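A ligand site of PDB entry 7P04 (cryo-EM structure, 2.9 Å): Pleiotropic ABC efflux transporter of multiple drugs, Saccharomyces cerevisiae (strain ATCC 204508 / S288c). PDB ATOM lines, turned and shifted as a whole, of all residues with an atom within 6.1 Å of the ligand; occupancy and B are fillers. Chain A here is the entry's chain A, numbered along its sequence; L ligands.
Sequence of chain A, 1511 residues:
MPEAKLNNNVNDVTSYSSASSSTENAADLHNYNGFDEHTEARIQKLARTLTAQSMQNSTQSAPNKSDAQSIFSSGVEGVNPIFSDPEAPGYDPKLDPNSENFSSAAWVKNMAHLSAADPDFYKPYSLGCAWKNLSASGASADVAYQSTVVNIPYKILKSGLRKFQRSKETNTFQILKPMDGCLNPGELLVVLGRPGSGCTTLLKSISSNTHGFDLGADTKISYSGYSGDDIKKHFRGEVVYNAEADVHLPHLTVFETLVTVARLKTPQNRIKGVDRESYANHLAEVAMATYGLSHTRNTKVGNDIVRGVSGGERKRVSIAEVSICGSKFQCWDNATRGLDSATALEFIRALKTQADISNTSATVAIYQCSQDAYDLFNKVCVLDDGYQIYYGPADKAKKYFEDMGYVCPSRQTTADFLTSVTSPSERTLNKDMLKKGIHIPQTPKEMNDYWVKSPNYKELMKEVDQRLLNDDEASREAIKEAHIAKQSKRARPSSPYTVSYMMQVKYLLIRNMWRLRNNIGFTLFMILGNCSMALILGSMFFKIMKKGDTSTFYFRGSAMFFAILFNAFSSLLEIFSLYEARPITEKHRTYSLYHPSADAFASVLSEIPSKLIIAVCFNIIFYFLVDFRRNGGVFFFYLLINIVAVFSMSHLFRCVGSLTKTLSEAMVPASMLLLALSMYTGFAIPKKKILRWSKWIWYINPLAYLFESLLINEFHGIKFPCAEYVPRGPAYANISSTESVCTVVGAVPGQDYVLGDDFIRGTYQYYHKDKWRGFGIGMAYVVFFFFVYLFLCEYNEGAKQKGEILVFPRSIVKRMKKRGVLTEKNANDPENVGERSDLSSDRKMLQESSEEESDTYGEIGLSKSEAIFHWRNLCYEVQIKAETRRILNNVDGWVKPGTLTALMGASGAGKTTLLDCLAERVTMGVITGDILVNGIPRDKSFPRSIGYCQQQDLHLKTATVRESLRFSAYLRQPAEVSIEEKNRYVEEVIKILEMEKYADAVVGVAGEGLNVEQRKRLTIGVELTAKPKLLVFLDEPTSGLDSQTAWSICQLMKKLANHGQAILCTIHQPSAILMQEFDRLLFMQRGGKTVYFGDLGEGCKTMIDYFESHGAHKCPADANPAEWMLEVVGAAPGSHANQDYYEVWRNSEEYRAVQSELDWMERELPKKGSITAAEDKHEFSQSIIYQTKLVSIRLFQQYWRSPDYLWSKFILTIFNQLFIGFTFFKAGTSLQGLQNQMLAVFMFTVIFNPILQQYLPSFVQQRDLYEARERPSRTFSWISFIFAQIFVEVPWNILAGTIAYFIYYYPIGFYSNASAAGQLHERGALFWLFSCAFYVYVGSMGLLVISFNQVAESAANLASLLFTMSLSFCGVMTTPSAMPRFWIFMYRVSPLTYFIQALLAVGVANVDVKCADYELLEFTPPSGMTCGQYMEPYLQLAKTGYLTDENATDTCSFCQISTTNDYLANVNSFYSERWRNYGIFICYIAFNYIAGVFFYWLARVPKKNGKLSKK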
ATOM      1  N   TYR A 876     -25.643 -22.393   2.769  1.00  0.00           N
ATOM      2  CA  TYR A 876     -24.601 -21.398   2.958  1.00  0.00           C
ATOM      3  C   TYR A 876     -25.218 -20.067   3.344  1.00  0.00           C
ATOM      4  O   TYR A 876     -26.265 -19.688   2.825  1.00  0.00           O
ATOM      5  CB  TYR A 876     -23.760 -21.248   1.686  1.00  0.00           C
ATOM      6  CG  TYR A 876     -22.629 -20.274   1.806  1.00  0.00           C
ATOM      7  CD1 TYR A 876     -21.513 -20.576   2.568  1.00  0.00           C
ATOM      8  CD2 TYR A 876     -22.653 -19.059   1.132  1.00  0.00           C
ATOM      9  CE1 TYR A 876     -20.458 -19.691   2.668  1.00  0.00           C
ATOM     10  CE2 TYR A 876     -21.607 -18.169   1.233  1.00  0.00           C
ATOM     11  CZ  TYR A 876     -20.513 -18.490   2.003  1.00  0.00           C
ATOM     12  OH  TYR A 876     -19.469 -17.604   2.112  1.00  0.00           O
ATOM     13  N   VAL A 878     -24.296 -15.804   4.875  1.00  0.00           N
ATOM     14  CA  VAL A 878     -23.370 -14.715   5.131  1.00  0.00           C
ATOM     15  C   VAL A 878     -24.063 -13.679   6.014  1.00  0.00           C
ATOM     16  O   VAL A 878     -25.246 -13.787   6.305  1.00  0.00           O
ATOM     17  CB  VAL A 878     -22.842 -14.067   3.834  1.00  0.00           C
ATOM     18  CG1 VAL A 878     -21.937 -15.030   3.090  1.00  0.00           C
ATOM     19  CG2 VAL A 878     -24.001 -13.627   2.948  1.00  0.00           C
ATOM     20  N   GLN A 879     -23.289 -12.668   6.422  1.00  0.00           N
ATOM     21  CA  GLN A 879     -23.823 -11.614   7.273  1.00  0.00           C
ATOM     22  C   GLN A 879     -23.407 -10.223   6.817  1.00  0.00           C
ATOM     23  O   GLN A 879     -23.542  -9.274   7.599  1.00  0.00           O
ATOM     24  CB  GLN A 879     -23.372 -11.829   8.724  1.00  0.00           C
ATOM     25  CG  GLN A 879     -23.994 -13.039   9.398  1.00  0.00           C
ATOM     26  CD  GLN A 879     -23.672 -13.102  10.885  1.00  0.00           C
ATOM     27  OE1 GLN A 879     -22.859 -12.329  11.386  1.00  0.00           O
ATOM     28  NE2 GLN A 879     -24.319 -14.019  11.592  1.00  0.00           N
ATOM     29  N   ILE A 880     -22.917 -10.063   5.588  1.00  0.00           N
ATOM     30  CA  ILE A 880     -22.392  -8.783   5.136  1.00  0.00           C
ATOM     31  C   ILE A 880     -23.518  -7.936   4.544  1.00  0.00           C
ATOM     32  O   ILE A 880     -23.820  -6.853   5.064  1.00  0.00           O
ATOM     33  CB  ILE A 880     -21.261  -8.974   4.117  1.00  0.00           C
ATOM     34  CG1 ILE A 880     -19.969  -9.407   4.831  1.00  0.00           C
ATOM     35  CG2 ILE A 880     -21.032  -7.710   3.302  1.00  0.00           C
ATOM     36  CD1 ILE A 880     -19.290  -8.296   5.616  1.00  0.00           C
ATOM     37  N   LYS A 881     -24.128  -8.426   3.468  1.00  0.00           N
ATOM     38  CA  LYS A 881     -25.197  -7.676   2.826  1.00  0.00           C
ATOM     39  C   LYS A 881     -26.506  -7.746   3.593  1.00  0.00           C
ATOM     40  O   LYS A 881     -27.421  -6.965   3.321  1.00  0.00           O
ATOM     41  CB  LYS A 881     -25.418  -8.181   1.401  1.00  0.00           C
ATOM     42  CG  LYS A 881     -26.548  -7.487   0.657  1.00  0.00           C
ATOM     43  CD  LYS A 881     -26.314  -7.483  -0.847  1.00  0.00           C
ATOM     44  CE  LYS A 881     -25.474  -6.300  -1.283  1.00  0.00           C
ATOM     45  NZ  LYS A 881     -25.242  -6.283  -2.746  1.00  0.00           N
ATOM     46  N   ARG A 885     -27.887 -13.909   5.277  1.00  0.00           N
ATOM     47  CA  ARG A 885     -28.380 -13.893   3.895  1.00  0.00           C
ATOM     48  C   ARG A 885     -27.953 -15.183   3.205  1.00  0.00           C
ATOM     49  O   ARG A 885     -26.754 -15.413   2.994  1.00  0.00           O
ATOM     50  CB  ARG A 885     -27.829 -12.680   3.159  1.00  0.00           C
ATOM     51  CG  ARG A 885     -28.210 -12.561   1.686  1.00  0.00           C
ATOM     52  CD  ARG A 885     -27.802 -11.196   1.156  1.00  0.00           C
ATOM     53  NE  ARG A 885     -27.893 -11.078  -0.301  1.00  0.00           N
ATOM     54  CZ  ARG A 885     -26.894 -11.334  -1.145  1.00  0.00           C
ATOM     55  NH1 ARG A 885     -25.708 -11.727  -0.691  1.00  0.00           N
ATOM     56  NH2 ARG A 885     -27.088 -11.188  -2.451  1.00  0.00           N
ATOM     57  N   ARG A 886     -28.923 -16.021   2.861  1.00  0.00           N
ATOM     58  CA  ARG A 886     -28.630 -17.311   2.253  1.00  0.00           C
ATOM     59  C   ARG A 886     -28.198 -17.132   0.810  1.00  0.00           C
ATOM     60  O   ARG A 886     -28.740 -16.305   0.078  1.00  0.00           O
ATOM     61  CB  ARG A 886     -29.839 -18.239   2.334  1.00  0.00           C
ATOM     62  CG  ARG A 886     -29.822 -19.157   3.534  1.00  0.00           C
ATOM     63  CD  ARG A 886     -30.816 -20.293   3.387  1.00  0.00           C
ATOM     64  NE  ARG A 886     -30.661 -21.295   4.426  1.00  0.00           N
ATOM     65  CZ  ARG A 886     -31.232 -22.491   4.401  1.00  0.00           C
ATOM     66  NH1 ARG A 886     -32.019 -22.835   3.392  1.00  0.00           N
ATOM     67  NH2 ARG A 886     -31.041 -23.350   5.398  1.00  0.00           N
ATOM     68  N   ILE A 887     -27.210 -17.924   0.399  1.00  0.00           N
ATOM     69  CA  ILE A 887     -26.739 -17.902  -0.989  1.00  0.00           C
ATOM     70  C   ILE A 887     -26.694 -19.277  -1.626  1.00  0.00           C
ATOM     71  O   ILE A 887     -26.622 -19.377  -2.854  1.00  0.00           O
ATOM     72  CB  ILE A 887     -25.345 -17.232  -1.080  1.00  0.00           C
ATOM     73  CG1 ILE A 887     -25.348 -15.895  -0.326  1.00  0.00           C
ATOM     74  CG2 ILE A 887     -24.967 -17.006  -2.522  1.00  0.00           C
ATOM     75  CD1 ILE A 887     -23.965 -15.380  -0.002  1.00  0.00           C
ATOM     76  N   GLY A 905     -26.922 -21.718 -14.496  1.00  0.00           N
ATOM     77  CA  GLY A 905     -27.782 -20.770 -13.830  1.00  0.00           C
ATOM     78  C   GLY A 905     -27.398 -19.359 -14.226  1.00  0.00           C
ATOM     79  O   GLY A 905     -26.256 -19.058 -14.564  1.00  0.00           O
ATOM     80  N   ALA A 906     -28.390 -18.478 -14.198  1.00  0.00           N
ATOM     81  CA  ALA A 906     -28.139 -17.082 -14.531  1.00  0.00           C
ATOM     82  C   ALA A 906     -27.135 -16.484 -13.552  1.00  0.00           C
ATOM     83  O   ALA A 906     -26.775 -17.095 -12.531  1.00  0.00           O
ATOM     84  CB  ALA A 906     -29.437 -16.290 -14.512  1.00  0.00           C
ATOM     85  N   SER A 907     -26.663 -15.286 -13.876  1.00  0.00           N
ATOM     86  CA  SER A 907     -25.749 -14.577 -12.977  1.00  0.00           C
ATOM     87  C   SER A 907     -26.309 -14.616 -11.563  1.00  0.00           C
ATOM     88  O   SER A 907     -27.526 -14.536 -11.355  1.00  0.00           O
ATOM     89  CB  SER A 907     -25.559 -13.135 -13.441  1.00  0.00           C
ATOM     90  OG  SER A 907     -24.709 -12.434 -12.551  1.00  0.00           O
ATOM     91  N   GLY A 908     -25.417 -14.726 -10.582  1.00  0.00           N
ATOM     92  CA  GLY A 908     -25.840 -15.078  -9.252  1.00  0.00           C
ATOM     93  C   GLY A 908     -26.082 -16.574  -9.178  1.00  0.00           C
ATOM     94  O   GLY A 908     -25.360 -17.367  -9.786  1.00  0.00           O
ATOM     95  N   ALA A 909     -27.105 -16.987  -8.428  1.00  0.00           N
ATOM     96  CA  ALA A 909     -27.451 -18.395  -8.230  1.00  0.00           C
ATOM     97  C   ALA A 909     -26.319 -19.176  -7.578  1.00  0.00           C
ATOM     98  O   ALA A 909     -26.386 -20.411  -7.507  1.00  0.00           O
ATOM     99  CB  ALA A 909     -27.840 -19.058  -9.551  1.00  0.00           C
ATOM    100  N   GLY A 910     -25.274 -18.501  -7.105  1.00  0.00           N
ATOM    101  CA  GLY A 910     -24.226 -19.157  -6.362  1.00  0.00           C
ATOM    102  C   GLY A 910     -23.485 -20.241  -7.119  1.00  0.00           C
ATOM    103  O   GLY A 910     -23.058 -21.214  -6.505  1.00  0.00           O
ATOM    104  N   LYS A 911     -23.317 -20.109  -8.433  1.00  0.00           N
ATOM    105  CA  LYS A 911     -22.479 -21.050  -9.147  1.00  0.00           C
ATOM    106  C   LYS A 911     -21.044 -20.981  -8.640  1.00  0.00           C
ATOM    107  O   LYS A 911     -20.484 -21.975  -8.154  1.00  0.00           O
ATOM    108  CB  LYS A 911     -22.528 -20.777 -10.650  1.00  0.00           C
ATOM    109  CG  LYS A 911     -23.921 -20.765 -11.254  1.00  0.00           C
ATOM    110  CD  LYS A 911     -23.874 -20.724 -12.763  1.00  0.00           C
ATOM    111  CE  LYS A 911     -23.051 -19.560 -13.294  1.00  0.00           C
ATOM    112  NZ  LYS A 911     -23.499 -18.251 -12.773  1.00  0.00           N
ATOM    113  N   THR A 912     -20.439 -19.796  -8.728  1.00  0.00           N
ATOM    114  CA  THR A 912     -19.117 -19.608  -8.152  1.00  0.00           C
ATOM    115  C   THR A 912     -19.158 -19.819  -6.639  1.00  0.00           C
ATOM    116  O   THR A 912     -18.212 -20.357  -6.056  1.00  0.00           O
ATOM    117  CB  THR A 912     -18.606 -18.204  -8.473  1.00  0.00           C
ATOM    118  OG1 THR A 912     -18.505 -18.040  -9.892  1.00  0.00           O
ATOM    119  CG2 THR A 912     -17.234 -17.977  -7.841  1.00  0.00           C
ATOM    120  N   THR A 913     -20.247 -19.421  -5.998  1.00  0.00           N
ATOM    121  CA  THR A 913     -20.379 -19.620  -4.559  1.00  0.00           C
ATOM    122  C   THR A 913     -20.402 -21.105  -4.203  1.00  0.00           C
ATOM    123  O   THR A 913     -19.743 -21.532  -3.264  1.00  0.00           O
ATOM    124  CB  THR A 913     -21.638 -18.927  -4.037  1.00  0.00           C
ATOM    125  OG1 THR A 913     -21.644 -17.565  -4.466  1.00  0.00           O
ATOM    126  CG2 THR A 913     -21.691 -18.980  -2.525  1.00  0.00           C
ATOM    127  N   LEU A 914     -21.172 -21.900  -4.949  1.00  0.00           N
ATOM    128  CA  LEU A 914     -21.208 -23.337  -4.710  1.00  0.00           C
ATOM    129  C   LEU A 914     -19.859 -23.977  -4.995  1.00  0.00           C
ATOM    130  O   LEU A 914     -19.420 -24.862  -4.262  1.00  0.00           O
ATOM    131  CB  LEU A 914     -22.310 -23.977  -5.539  1.00  0.00           C
ATOM    132  CG  LEU A 914     -22.290 -25.508  -5.591  1.00  0.00           C
ATOM    133  CD1 LEU A 914     -22.404 -26.073  -4.191  1.00  0.00           C
ATOM    134  CD2 LEU A 914     -23.420 -26.016  -6.450  1.00  0.00           C
ATOM    135  N   ASP A 916     -16.979 -22.583  -4.683  1.00  0.00           N
ATOM    136  CA  ASP A 916     -16.094 -22.220  -3.592  1.00  0.00           C
ATOM    137  C   ASP A 916     -16.438 -22.988  -2.323  1.00  0.00           C
ATOM    138  O   ASP A 916     -15.534 -23.394  -1.577  1.00  0.00           O
ATOM    139  CB  ASP A 916     -16.168 -20.719  -3.349  1.00  0.00           C
ATOM    140  CG  ASP A 916     -15.709 -19.919  -4.549  1.00  0.00           C
ATOM    141  OD1 ASP A 916     -14.850 -20.423  -5.304  1.00  0.00           O
ATOM    142  OD2 ASP A 916     -16.200 -18.795  -4.751  1.00  0.00           O
ATOM    143  N   MET A 924     -15.774 -16.210   4.442  1.00  0.00           N
ATOM    144  CA  MET A 924     -16.929 -15.630   5.116  1.00  0.00           C
ATOM    145  C   MET A 924     -18.092 -16.611   5.112  1.00  0.00           C
ATOM    146  O   MET A 924     -18.142 -17.561   4.340  1.00  0.00           O
ATOM    147  CB  MET A 924     -17.342 -14.329   4.448  1.00  0.00           C
ATOM    148  CG  MET A 924     -17.916 -14.508   3.046  1.00  0.00           C
ATOM    149  SD  MET A 924     -18.015 -12.980   2.102  1.00  0.00           S
ATOM    150  CE  MET A 924     -16.272 -12.612   1.860  1.00  0.00           C
ATOM    151  N   GLN A 951     -11.840 -18.334 -12.896  1.00  0.00           N
ATOM    152  CA  GLN A 951     -12.319 -17.729 -14.136  1.00  0.00           C
ATOM    153  C   GLN A 951     -11.322 -16.705 -14.662  1.00  0.00           C
ATOM    154  O   GLN A 951     -10.911 -16.748 -15.821  1.00  0.00           O
ATOM    155  CB  GLN A 951     -13.691 -17.102 -13.910  1.00  0.00           C
ATOM    156  CG  GLN A 951     -14.354 -16.611 -15.176  1.00  0.00           C
ATOM    157  CD  GLN A 951     -15.434 -15.588 -14.897  1.00  0.00           C
ATOM    158  OE1 GLN A 951     -15.478 -14.532 -15.521  1.00  0.00           O
ATOM    159  NE2 GLN A 951     -16.307 -15.901 -13.952  1.00  0.00           N
ATOM    160  N   ASP A1035     -14.204 -22.785 -13.131  1.00  0.00           N
ATOM    161  CA  ASP A1035     -15.140 -21.672 -13.093  1.00  0.00           C
ATOM    162  C   ASP A1035     -15.153 -21.029 -14.472  1.00  0.00           C
ATOM    163  O   ASP A1035     -14.121 -20.508 -14.931  1.00  0.00           O
ATOM    164  CB  ASP A1035     -14.765 -20.671 -12.014  1.00  0.00           C
ATOM    165  CG  ASP A1035     -15.923 -19.771 -11.624  1.00  0.00           C
ATOM    166  OD1 ASP A1035     -17.072 -20.123 -11.941  1.00  0.00           O
ATOM    167  OD2 ASP A1035     -15.682 -18.718 -11.016  1.00  0.00           O
ATOM    168  N   GLU A1036     -16.307 -21.060 -15.131  1.00  0.00           N
ATOM    169  CA  GLU A1036     -16.561 -20.402 -16.413  1.00  0.00           C
ATOM    170  C   GLU A1036     -15.325 -20.466 -17.315  1.00  0.00           C
ATOM    171  O   GLU A1036     -14.767 -19.434 -17.693  1.00  0.00           O
ATOM    172  CB  GLU A1036     -17.007 -18.961 -16.204  1.00  0.00           C
ATOM    173  CG  GLU A1036     -18.482 -18.813 -15.922  1.00  0.00           C
ATOM    174  CD  GLU A1036     -18.902 -17.360 -15.793  1.00  0.00           C
ATOM    175  OE1 GLU A1036     -18.300 -16.503 -16.472  1.00  0.00           O
ATOM    176  OE2 GLU A1036     -19.831 -17.078 -15.010  1.00  0.00           O
ATOM    177  N   THR A1066     -18.332 -24.786 -14.130  1.00  0.00           N
ATOM    178  CA  THR A1066     -19.428 -23.834 -14.229  1.00  0.00           C
ATOM    179  C   THR A1066     -19.475 -23.267 -15.646  1.00  0.00           C
ATOM    180  O   THR A1066     -18.458 -22.845 -16.184  1.00  0.00           O
ATOM    181  CB  THR A1066     -19.265 -22.714 -13.211  1.00  0.00           C
ATOM    182  OG1 THR A1066     -19.534 -23.218 -11.900  1.00  0.00           O
ATOM    183  CG2 THR A1066     -20.201 -21.569 -13.516  1.00  0.00           C
HETATM  184  P1  LIG L   1     -22.010 -16.198 -10.343  1.00  0.00           P
HETATM  185  O1  LIG L   1     -22.752 -17.477 -10.073  1.00  0.00           O
HETATM  186  O2  LIG L   1     -22.869 -14.957 -10.264  1.00  0.00           O
HETATM  187  O3  LIG L   1     -21.058 -16.225 -11.518  1.00  0.00           O
HETATM  188  P2  LIG L   1     -21.706 -16.248  -7.612  1.00  0.00           P
HETATM  189  O4  LIG L   1     -21.535 -17.667  -7.149  1.00  0.00           O
HETATM  190  O5  LIG L   1     -23.086 -15.668  -7.668  1.00  0.00           O
HETATM  191  O6  LIG L   1     -21.051 -16.064  -9.064  1.00  0.00           O
HETATM  192  O7  LIG L   1     -20.816 -15.282  -6.688  1.00  0.00           O
HETATM  193  C1  LIG L   1     -21.417 -14.069  -6.245  1.00  0.00           C
HETATM  194  C2  LIG L   1     -22.413 -14.371  -5.127  1.00  0.00           C
HETATM  195  O8  LIG L   1     -21.759 -14.301  -3.856  1.00  0.00           O
HETATM  196  C3  LIG L   1     -23.551 -13.361  -5.114  1.00  0.00           C
HETATM  197  O9  LIG L   1     -24.719 -13.917  -5.730  1.00  0.00           O
HETATM  198  C4  LIG L   1     -23.786 -13.065  -3.648  1.00  0.00           C
HETATM  199  O10 LIG L   1     -24.913 -13.792  -3.161  1.00  0.00           O
HETATM  200  C5  LIG L   1     -22.511 -13.509  -2.943  1.00  0.00           C
HETATM  201  N1  LIG L   1     -21.698 -12.325  -2.584  1.00  0.00           N
HETATM  202  C6  LIG L   1     -21.182 -11.457  -3.478  1.00  0.00           C
HETATM  203  N2  LIG L   1     -20.486 -10.479  -2.852  1.00  0.00           N
HETATM  204  C7  LIG L   1     -20.554 -10.717  -1.534  1.00  0.00           C
HETATM  205  C8  LIG L   1     -20.025 -10.062  -0.309  1.00  0.00           C
HETATM  206  N3  LIG L   1     -19.281  -8.937  -0.394  1.00  0.00           N
HETATM  207  N4  LIG L   1     -20.316 -10.632   0.881  1.00  0.00           N
HETATM  208  C9  LIG L   1     -21.061 -11.760   0.974  1.00  0.00           C
HETATM  209  N5  LIG L   1     -21.560 -12.398  -0.106  1.00  0.00           N
HETATM  210  C10 LIG L   1     -21.348 -11.938  -1.362  1.00  0.00           C
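N of Thr 913 lies within hydrogen-bond range of O4 of the ligand, 2.5 Å away.
The side-chain hydroxyl of Thr 913 sits at hydrogen-bond distance from an oxygen (O4) of the ligand (2.7 Å).
N of Gly 908 is in hydrogen-bond range of O2 of the ligand (2.6 Å).
The backbone carbonyl oxygen (O) of Gly 908 sits close to an oxygen (O1) of the ligand (2.6 Å).
N of Thr 912 sits at hydrogen-bond distance from O4 of the ligand, at 2.9 Å.
The side-chain hydroxyl (OG1) of Thr 912 sits close to an oxygen (O6) of the ligand (3.3 Å).
An oxygen (O1) of the ligand sits at hydrogen-bond distance from the backbone NH of Lys 911, 3.2 Å away.
NZ of Lys 911 lies within salt-bridge range of O1 of the ligand (2.9 Å).
NH1 of Arg 885 sits at hydrogen-bond distance from O10 of the ligand.
A nitrogen (N4) of the ligand sits close to the side-chain sulfur (SD) of Met 924, at 3.5 Å.
Merely in contact with the ligand: Gly 910 (3.2 Å), Ile 887 (3.3 Å), Ser 907 (3.7 Å), Ile 880 (3.8 Å), Glu 1036 (3.8 Å) and Val 878 (3.99 Å).
Of the 24 residues printed, 12 come within 4 Å of the ligand.
OD2 of Asp 1035 sits at hydrogen-bond distance from OG1 of Thr 912, at 3.1 Å.
O of Ala 906 is in hydrogen-bond range of NZ of Lys 911, 3.5 Å away.
NZ of Lys 911 is in hydrogen-bond range of O of Gly 905 (3.4 Å).
The backbone NH (N) of Ile 887 is in hydrogen-bond range of the backbone carbonyl oxygen (O) of Tyr 876, 3.1 Å away.
The backbone carbonyl oxygen of Val 878 is in hydrogen-bond range of the backbone NH of Arg 885.
The side-chain hydroxyl (OH) of Tyr 876 is in hydrogen-bond range of the backbone carbonyl oxygen (O) of Met 924 (2.6 Å).
OE1 of Glu 1036 is in hydrogen-bond range of NE2 of Gln 951, at 3.3 Å.
O of Thr 1066 sits at hydrogen-bond distance from N of Glu 1036 (3.0 Å).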
